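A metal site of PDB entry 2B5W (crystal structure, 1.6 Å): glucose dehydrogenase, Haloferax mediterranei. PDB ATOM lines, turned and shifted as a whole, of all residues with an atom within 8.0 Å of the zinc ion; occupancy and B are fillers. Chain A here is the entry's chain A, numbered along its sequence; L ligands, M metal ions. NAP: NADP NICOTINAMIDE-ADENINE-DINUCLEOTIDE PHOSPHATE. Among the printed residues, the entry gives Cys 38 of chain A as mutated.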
ATOM      1  N   GLY A  36      -0.957  -9.413 -33.462  1.00  0.00           N
ATOM      2  CA  GLY A  36      -1.035  -9.112 -32.065  1.00  0.00           C
ATOM      3  C   GLY A  36       0.214  -8.511 -31.471  1.00  0.00           C
ATOM      4  O   GLY A  36       1.293  -8.566 -32.060  1.00  0.00           O
ATOM      5  N   VAL A  37       0.050  -7.902 -30.309  1.00  0.00           N
ATOM      6  CA  VAL A  37       1.127  -7.327 -29.521  1.00  0.00           C
ATOM      7  C   VAL A  37       1.131  -8.028 -28.161  1.00  0.00           C
ATOM      8  O   VAL A  37       0.081  -8.298 -27.586  1.00  0.00           O
ATOM      9  CB  VAL A  37       0.901  -5.837 -29.355  1.00  0.00           C
ATOM     10  CG1 VAL A  37       1.936  -5.207 -28.426  1.00  0.00           C
ATOM     11  CG2 VAL A  37       0.896  -5.122 -30.713  1.00  0.00           C
ATOM     12  N   CYS A  38       2.282  -8.467 -27.668  1.00  0.00           N
ATOM     13  CA  CYS A  38       2.353  -9.005 -26.311  1.00  0.00           C
ATOM     14  C   CYS A  38       3.576  -8.461 -25.595  1.00  0.00           C
ATOM     15  O   CYS A  38       4.303  -7.636 -26.144  1.00  0.00           O
ATOM     16  CB  CYS A  38       2.365 -10.533 -26.271  1.00  0.00           C
ATOM     17  SG  CYS A  38       3.965 -11.315 -26.639  1.00  0.00           S
ATOM     18  N   GLY A  39       3.803  -8.958 -24.388  1.00  0.00           N
ATOM     19  CA  GLY A  39       4.919  -8.473 -23.589  1.00  0.00           C
ATOM     20  C   GLY A  39       6.235  -8.588 -24.321  1.00  0.00           C
ATOM     21  O   GLY A  39       7.103  -7.736 -24.209  1.00  0.00           O
ATOM     22  N   THR A  40       6.392  -9.670 -25.081  1.00  0.00           N
ATOM     23  CA  THR A  40       7.603  -9.839 -25.859  1.00  0.00           C
ATOM     24  C   THR A  40       7.879  -8.647 -26.752  1.00  0.00           C
ATOM     25  O   THR A  40       9.022  -8.235 -26.943  1.00  0.00           O
ATOM     26  CB  THR A  40       7.521 -11.128 -26.745  1.00  0.00           C
ATOM     27  OG1 THR A  40       7.252 -12.291 -25.927  1.00  0.00           O
ATOM     28  CG2 THR A  40       8.880 -11.403 -27.403  1.00  0.00           C
ATOM     29  N   ASP A  41       6.856  -8.131 -27.417  1.00  0.00           N
ATOM     30  CA  ASP A  41       7.024  -6.930 -28.275  1.00  0.00           C
ATOM     31  C   ASP A  41       7.496  -5.713 -27.490  1.00  0.00           C
ATOM     32  O   ASP A  41       8.323  -4.922 -27.970  1.00  0.00           O
ATOM     33  CB  ASP A  41       5.692  -6.559 -28.968  1.00  0.00           C
ATOM     34  CG  ASP A  41       5.308  -7.544 -30.011  1.00  0.00           C
ATOM     35  OD1 ASP A  41       4.428  -8.385 -29.726  1.00  0.00           O
ATOM     36  OD2 ASP A  41       5.920  -7.525 -31.101  1.00  0.00           O
ATOM     37  N   GLY A  62       6.455  -7.862 -34.620  1.00  0.00           N
ATOM     38  CA  GLY A  62       5.283  -8.707 -34.683  1.00  0.00           C
ATOM     39  C   GLY A  62       5.605 -10.160 -34.932  1.00  0.00           C
ATOM     40  O   GLY A  62       6.178 -10.519 -35.972  1.00  0.00           O
ATOM     41  N   HIS A  63       5.137 -11.019 -34.033  1.00  0.00           N
ATOM     42  CA  HIS A  63       5.330 -12.463 -34.196  1.00  0.00           C
ATOM     43  C   HIS A  63       4.017 -13.231 -34.072  1.00  0.00           C
ATOM     44  O   HIS A  63       3.999 -14.446 -34.195  1.00  0.00           O
ATOM     45  CB  HIS A  63       6.332 -12.996 -33.148  1.00  0.00           C
ATOM     46  CG  HIS A  63       5.902 -12.716 -31.756  1.00  0.00           C
ATOM     47  ND1 HIS A  63       6.107 -11.489 -31.146  1.00  0.00           N
ATOM     48  CD2 HIS A  63       5.189 -13.465 -30.874  1.00  0.00           C
ATOM     49  CE1 HIS A  63       5.529 -11.494 -29.959  1.00  0.00           C
ATOM     50  NE2 HIS A  63       4.948 -12.671 -29.774  1.00  0.00           N
ATOM     51  N   GLU A  64       2.910 -12.543 -33.789  1.00  0.00           N
ATOM     52  CA  GLU A  64       1.588 -13.172 -33.635  1.00  0.00           C
ATOM     53  C   GLU A  64       0.656 -12.766 -34.793  1.00  0.00           C
ATOM     54  O   GLU A  64      -0.158 -11.825 -34.669  1.00  0.00           O
ATOM     55  CB  GLU A  64       0.959 -12.700 -32.342  1.00  0.00           C
ATOM     56  CG  GLU A  64       1.780 -12.816 -31.102  1.00  0.00           C
ATOM     57  CD  GLU A  64       1.091 -12.233 -29.896  1.00  0.00           C
ATOM     58  OE1 GLU A  64      -0.019 -11.684 -30.035  1.00  0.00           O
ATOM     59  OE2 GLU A  64       1.632 -12.394 -28.810  1.00  0.00           O
ATOM     60  N   VAL A  87       7.061 -18.919 -35.704  1.00  0.00           N
ATOM     61  CA  VAL A  87       7.976 -17.830 -35.428  1.00  0.00           C
ATOM     62  C   VAL A  87       9.429 -18.134 -35.774  1.00  0.00           C
ATOM     63  O   VAL A  87      10.159 -17.253 -36.237  1.00  0.00           O
ATOM     64  CB  VAL A  87       7.859 -17.440 -33.952  1.00  0.00           C
ATOM     65  CG1 VAL A  87       8.770 -16.279 -33.622  1.00  0.00           C
ATOM     66  CG2 VAL A  87       6.403 -17.027 -33.631  1.00  0.00           C
ATOM     67  N   ILE A 117      11.527 -10.696 -33.451  1.00  0.00           N
ATOM     68  CA  ILE A 117      12.113 -10.741 -32.122  1.00  0.00           C
ATOM     69  C   ILE A 117      13.646 -10.738 -32.185  1.00  0.00           C
ATOM     70  O   ILE A 117      14.282  -9.874 -31.585  1.00  0.00           O
ATOM     71  CB  ILE A 117      11.604 -11.962 -31.347  1.00  0.00           C
ATOM     72  CG1 ILE A 117      10.098 -11.941 -31.280  1.00  0.00           C
ATOM     73  CG2 ILE A 117      12.187 -11.952 -29.924  1.00  0.00           C
ATOM     74  CD1 ILE A 117       9.506 -13.244 -30.692  1.00  0.00           C
ATOM     75  N   PHE A 147      -4.669 -13.856 -34.509  1.00  0.00           N
ATOM     76  CA  PHE A 147      -3.489 -13.445 -33.774  1.00  0.00           C
ATOM     77  C   PHE A 147      -3.370 -14.060 -32.395  1.00  0.00           C
ATOM     78  O   PHE A 147      -2.357 -13.868 -31.758  1.00  0.00           O
ATOM     79  CB  PHE A 147      -3.400 -11.911 -33.723  1.00  0.00           C
ATOM     80  CG  PHE A 147      -4.546 -11.268 -33.010  1.00  0.00           C
ATOM     81  CD1 PHE A 147      -4.510 -11.056 -31.626  1.00  0.00           C
ATOM     82  CD2 PHE A 147      -5.675 -10.851 -33.701  1.00  0.00           C
ATOM     83  CE1 PHE A 147      -5.595 -10.486 -30.992  1.00  0.00           C
ATOM     84  CE2 PHE A 147      -6.729 -10.300 -33.068  1.00  0.00           C
ATOM     85  CZ  PHE A 147      -6.707 -10.099 -31.730  1.00  0.00           C
ATOM     86  N   GLU A 150      -0.964 -17.955 -32.024  1.00  0.00           N
ATOM     87  CA  GLU A 150       0.393 -18.083 -31.537  1.00  0.00           C
ATOM     88  C   GLU A 150       0.513 -18.057 -30.012  1.00  0.00           C
ATOM     89  O   GLU A 150       1.139 -18.931 -29.432  1.00  0.00           O
ATOM     90  CB  GLU A 150       1.347 -17.070 -32.223  1.00  0.00           C
ATOM     91  CG  GLU A 150       2.843 -17.368 -32.001  1.00  0.00           C
ATOM     92  CD  GLU A 150       3.408 -16.803 -30.729  1.00  0.00           C
ATOM     93  OE1 GLU A 150       2.691 -16.022 -30.053  1.00  0.00           O
ATOM     94  OE2 GLU A 150       4.572 -17.128 -30.363  1.00  0.00           O
ATOM     95  N   PRO A 151      -0.066 -17.083 -29.289  1.00  0.00           N
ATOM     96  CA  PRO A 151      -0.010 -17.134 -27.830  1.00  0.00           C
ATOM     97  C   PRO A 151      -0.618 -18.403 -27.237  1.00  0.00           C
ATOM     98  O   PRO A 151      -0.065 -18.954 -26.297  1.00  0.00           O
ATOM     99  CB  PRO A 151      -0.808 -15.893 -27.402  1.00  0.00           C
ATOM    100  CG  PRO A 151      -0.960 -15.090 -28.548  1.00  0.00           C
ATOM    101  CD  PRO A 151      -0.601 -15.802 -29.802  1.00  0.00           C
ATOM    102  N   ILE A 154       1.895 -21.215 -27.431  1.00  0.00           N
ATOM    103  CA  ILE A 154       2.927 -21.130 -26.401  1.00  0.00           C
ATOM    104  C   ILE A 154       2.494 -21.973 -25.202  1.00  0.00           C
ATOM    105  O   ILE A 154       3.263 -22.760 -24.661  1.00  0.00           O
ATOM    106  CB  ILE A 154       3.211 -19.663 -26.000  1.00  0.00           C
ATOM    107  CG1 ILE A 154       3.839 -18.881 -27.153  1.00  0.00           C
ATOM    108  CG2 ILE A 154       4.017 -19.634 -24.734  1.00  0.00           C
ATOM    109  CD1 ILE A 154       5.157 -19.377 -27.617  1.00  0.00           C
ATOM    110  N   SER A 183      -1.553 -10.808 -20.827  1.00  0.00           N
ATOM    111  CA  SER A 183      -2.399 -11.548 -21.782  1.00  0.00           C
ATOM    112  C   SER A 183      -2.073 -13.046 -21.789  1.00  0.00           C
ATOM    113  O   SER A 183      -2.950 -13.861 -21.990  1.00  0.00           O
ATOM    114  CB  SER A 183      -2.330 -10.929 -23.184  1.00  0.00           C
ATOM    115  OG  SER A 183      -1.057 -11.012 -23.765  1.00  0.00           O
ATOM    116  N   LEU A 184      -0.809 -13.407 -21.629  1.00  0.00           N
ATOM    117  CA  LEU A 184      -0.464 -14.846 -21.634  1.00  0.00           C
ATOM    118  C   LEU A 184      -1.077 -15.583 -20.427  1.00  0.00           C
ATOM    119  O   LEU A 184      -1.683 -16.655 -20.539  1.00  0.00           O
ATOM    120  CB  LEU A 184       1.057 -15.063 -21.720  1.00  0.00           C
ATOM    121  CG  LEU A 184       1.480 -16.538 -21.809  1.00  0.00           C
ATOM    122  CD1 LEU A 184       0.911 -17.242 -23.052  1.00  0.00           C
ATOM    123  CD2 LEU A 184       3.004 -16.686 -21.720  1.00  0.00           C
ATOM    124  N   LYS A 349      -4.987  -7.262 -24.221  1.00  0.00           N
ATOM    125  CA  LYS A 349      -4.474  -7.717 -25.500  1.00  0.00           C
ATOM    126  C   LYS A 349      -4.921  -6.816 -26.645  1.00  0.00           C
ATOM    127  O   LYS A 349      -6.095  -6.511 -26.735  1.00  0.00           O
ATOM    128  CB  LYS A 349      -4.988  -9.127 -25.796  1.00  0.00           C
ATOM    129  CG  LYS A 349      -4.468  -9.725 -27.065  1.00  0.00           C
ATOM    130  CD  LYS A 349      -2.990 -10.014 -26.874  1.00  0.00           C
ATOM    131  CE  LYS A 349      -2.375 -10.694 -28.030  1.00  0.00           C
ATOM    132  NZ  LYS A 349      -0.948 -10.880 -27.700  1.00  0.00           N
HETATM  133  PA  NAP L   1       3.103  -9.061 -19.332  1.00  0.00           P
HETATM  134  O1A NAP L   1       4.185  -8.141 -19.014  1.00  0.00           O
HETATM  135  O2A NAP L   1       1.961  -8.408 -20.125  1.00  0.00           O
HETATM  136  O5B NAP L   1       2.473  -9.674 -18.019  1.00  0.00           O
HETATM  137  C5B NAP L   1       3.193  -9.990 -16.862  1.00  0.00           C
HETATM  138  C4B NAP L   1       2.175  -9.744 -15.768  1.00  0.00           C
HETATM  139  O4B NAP L   1       2.710 -10.259 -14.563  1.00  0.00           O
HETATM  140  C3B NAP L   1       1.845  -8.260 -15.551  1.00  0.00           C
HETATM  141  O3B NAP L   1       0.465  -7.966 -15.697  1.00  0.00           O
HETATM  142  C2B NAP L   1       2.329  -7.987 -14.126  1.00  0.00           C
HETATM  143  O2B NAP L   1       1.483  -7.169 -13.345  1.00  0.00           O
HETATM  144  C1B NAP L   1       2.386  -9.367 -13.517  1.00  0.00           C
HETATM  145  N9A NAP L   1       3.405  -9.461 -12.488  1.00  0.00           N
HETATM  146  C8A NAP L   1       4.751  -9.230 -12.632  1.00  0.00           C
HETATM  147  N7A NAP L   1       5.343  -9.411 -11.438  1.00  0.00           N
HETATM  148  C5A NAP L   1       4.365  -9.722 -10.520  1.00  0.00           C
HETATM  149  C6A NAP L   1       4.368 -10.004  -9.143  1.00  0.00           C
HETATM  150  N6A NAP L   1       5.481  -9.950  -8.397  1.00  0.00           N
HETATM  151  N1A NAP L   1       3.185 -10.298  -8.507  1.00  0.00           N
HETATM  152  C2A NAP L   1       1.998 -10.341  -9.211  1.00  0.00           C
HETATM  153  N3A NAP L   1       1.974 -10.063 -10.568  1.00  0.00           N
HETATM  154  C4A NAP L   1       3.133  -9.772 -11.199  1.00  0.00           C
HETATM  155  O3  NAP L   1       3.605 -10.217 -20.299  1.00  0.00           O
HETATM  156  PN  NAP L   1       2.806 -11.390 -21.082  1.00  0.00           P
HETATM  157  O1N NAP L   1       1.635 -11.889 -20.295  1.00  0.00           O
HETATM  158  O2N NAP L   1       2.639 -11.085 -22.537  1.00  0.00           O
HETATM  159  O5D NAP L   1       4.061 -12.333 -20.805  1.00  0.00           O
HETATM  160  C5D NAP L   1       4.255 -12.937 -19.549  1.00  0.00           C
HETATM  161  C4D NAP L   1       5.678 -13.475 -19.418  1.00  0.00           C
HETATM  162  O4D NAP L   1       5.822 -14.541 -20.363  1.00  0.00           O
HETATM  163  C3D NAP L   1       6.764 -12.451 -19.731  1.00  0.00           C
HETATM  164  O3D NAP L   1       7.854 -12.576 -18.839  1.00  0.00           O
HETATM  165  C2D NAP L   1       7.172 -12.814 -21.162  1.00  0.00           C
HETATM  166  O2D NAP L   1       8.451 -12.388 -21.543  1.00  0.00           O
HETATM  167  C1D NAP L   1       7.019 -14.334 -21.130  1.00  0.00           C
HETATM  168  N1N NAP L   1       6.744 -14.988 -22.409  1.00  0.00           N
HETATM  169  C2N NAP L   1       7.474 -16.110 -22.652  1.00  0.00           C
HETATM  170  C3N NAP L   1       7.231 -16.849 -23.766  1.00  0.00           C
HETATM  171  C7N NAP L   1       7.949 -18.164 -23.854  1.00  0.00           C
HETATM  172  O7N NAP L   1       7.812 -18.753 -25.107  1.00  0.00           O
HETATM  173  N7N NAP L   1       8.636 -18.640 -22.775  1.00  0.00           N
HETATM  174  C4N NAP L   1       6.284 -16.456 -24.723  1.00  0.00           C
HETATM  175  C5N NAP L   1       5.537 -15.309 -24.463  1.00  0.00           C
HETATM  176  C6N NAP L   1       5.758 -14.592 -23.289  1.00  0.00           C
HETATM  177  P2B NAP L   1       1.657  -5.521 -13.287  1.00  0.00           P
HETATM  178  O1X NAP L   1       1.352  -4.911 -14.554  1.00  0.00           O
HETATM  179  O2X NAP L   1       0.683  -5.125 -12.163  1.00  0.00           O
HETATM  180  O3X NAP L   1       3.095  -5.187 -12.880  1.00  0.00           O
HETATM  181 ZN    ZN M   1       3.423 -12.710 -28.372  1.00  0.00          ZN
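The backbone NH of Gly 39 is in hydrogen-bond range of an oxygen (O2N) of the ligand.
N of Leu 184 lies within hydrogen-bond range of O1N of the ligand (3.2 Å).
N of Ser 183 is in hydrogen-bond range of O1N of the ligand, at 3.4 Å.
The side-chain carboxylate (OE1) of Glu 64 is in salt-bridge range of the side-chain amino group (NZ) of Lys 349, 2.6 Å away.
The backbone NH (N) of Cys 38 is in hydrogen-bond range of the side-chain carboxylate (OD1) of Asp 41, at 3.0 Å.
The backbone carbonyl oxygen of Glu 64 sits at hydrogen-bond distance from the backbone NH of Gly 36 (2.8 Å).
SG of Cys 38 lies close to N of Thr 40 (3.3 Å).
Glu 150 touches the zinc ion (OE1 to ZN, 3.8 Å).
Within 4 Å of the zinc ion: Cys 38, His 63, Glu 64 and Glu 150.
OE2 of Glu 64 is bound to the zinc ion (1.9 Å).
NE2 of His 63 is bound to the zinc ion, 2.1 Å away.
The zinc ion is bound by the side-chain sulfur (SG) of Cys 38, 2.3 Å away.
The zinc ion has three donor atoms within binding distance.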
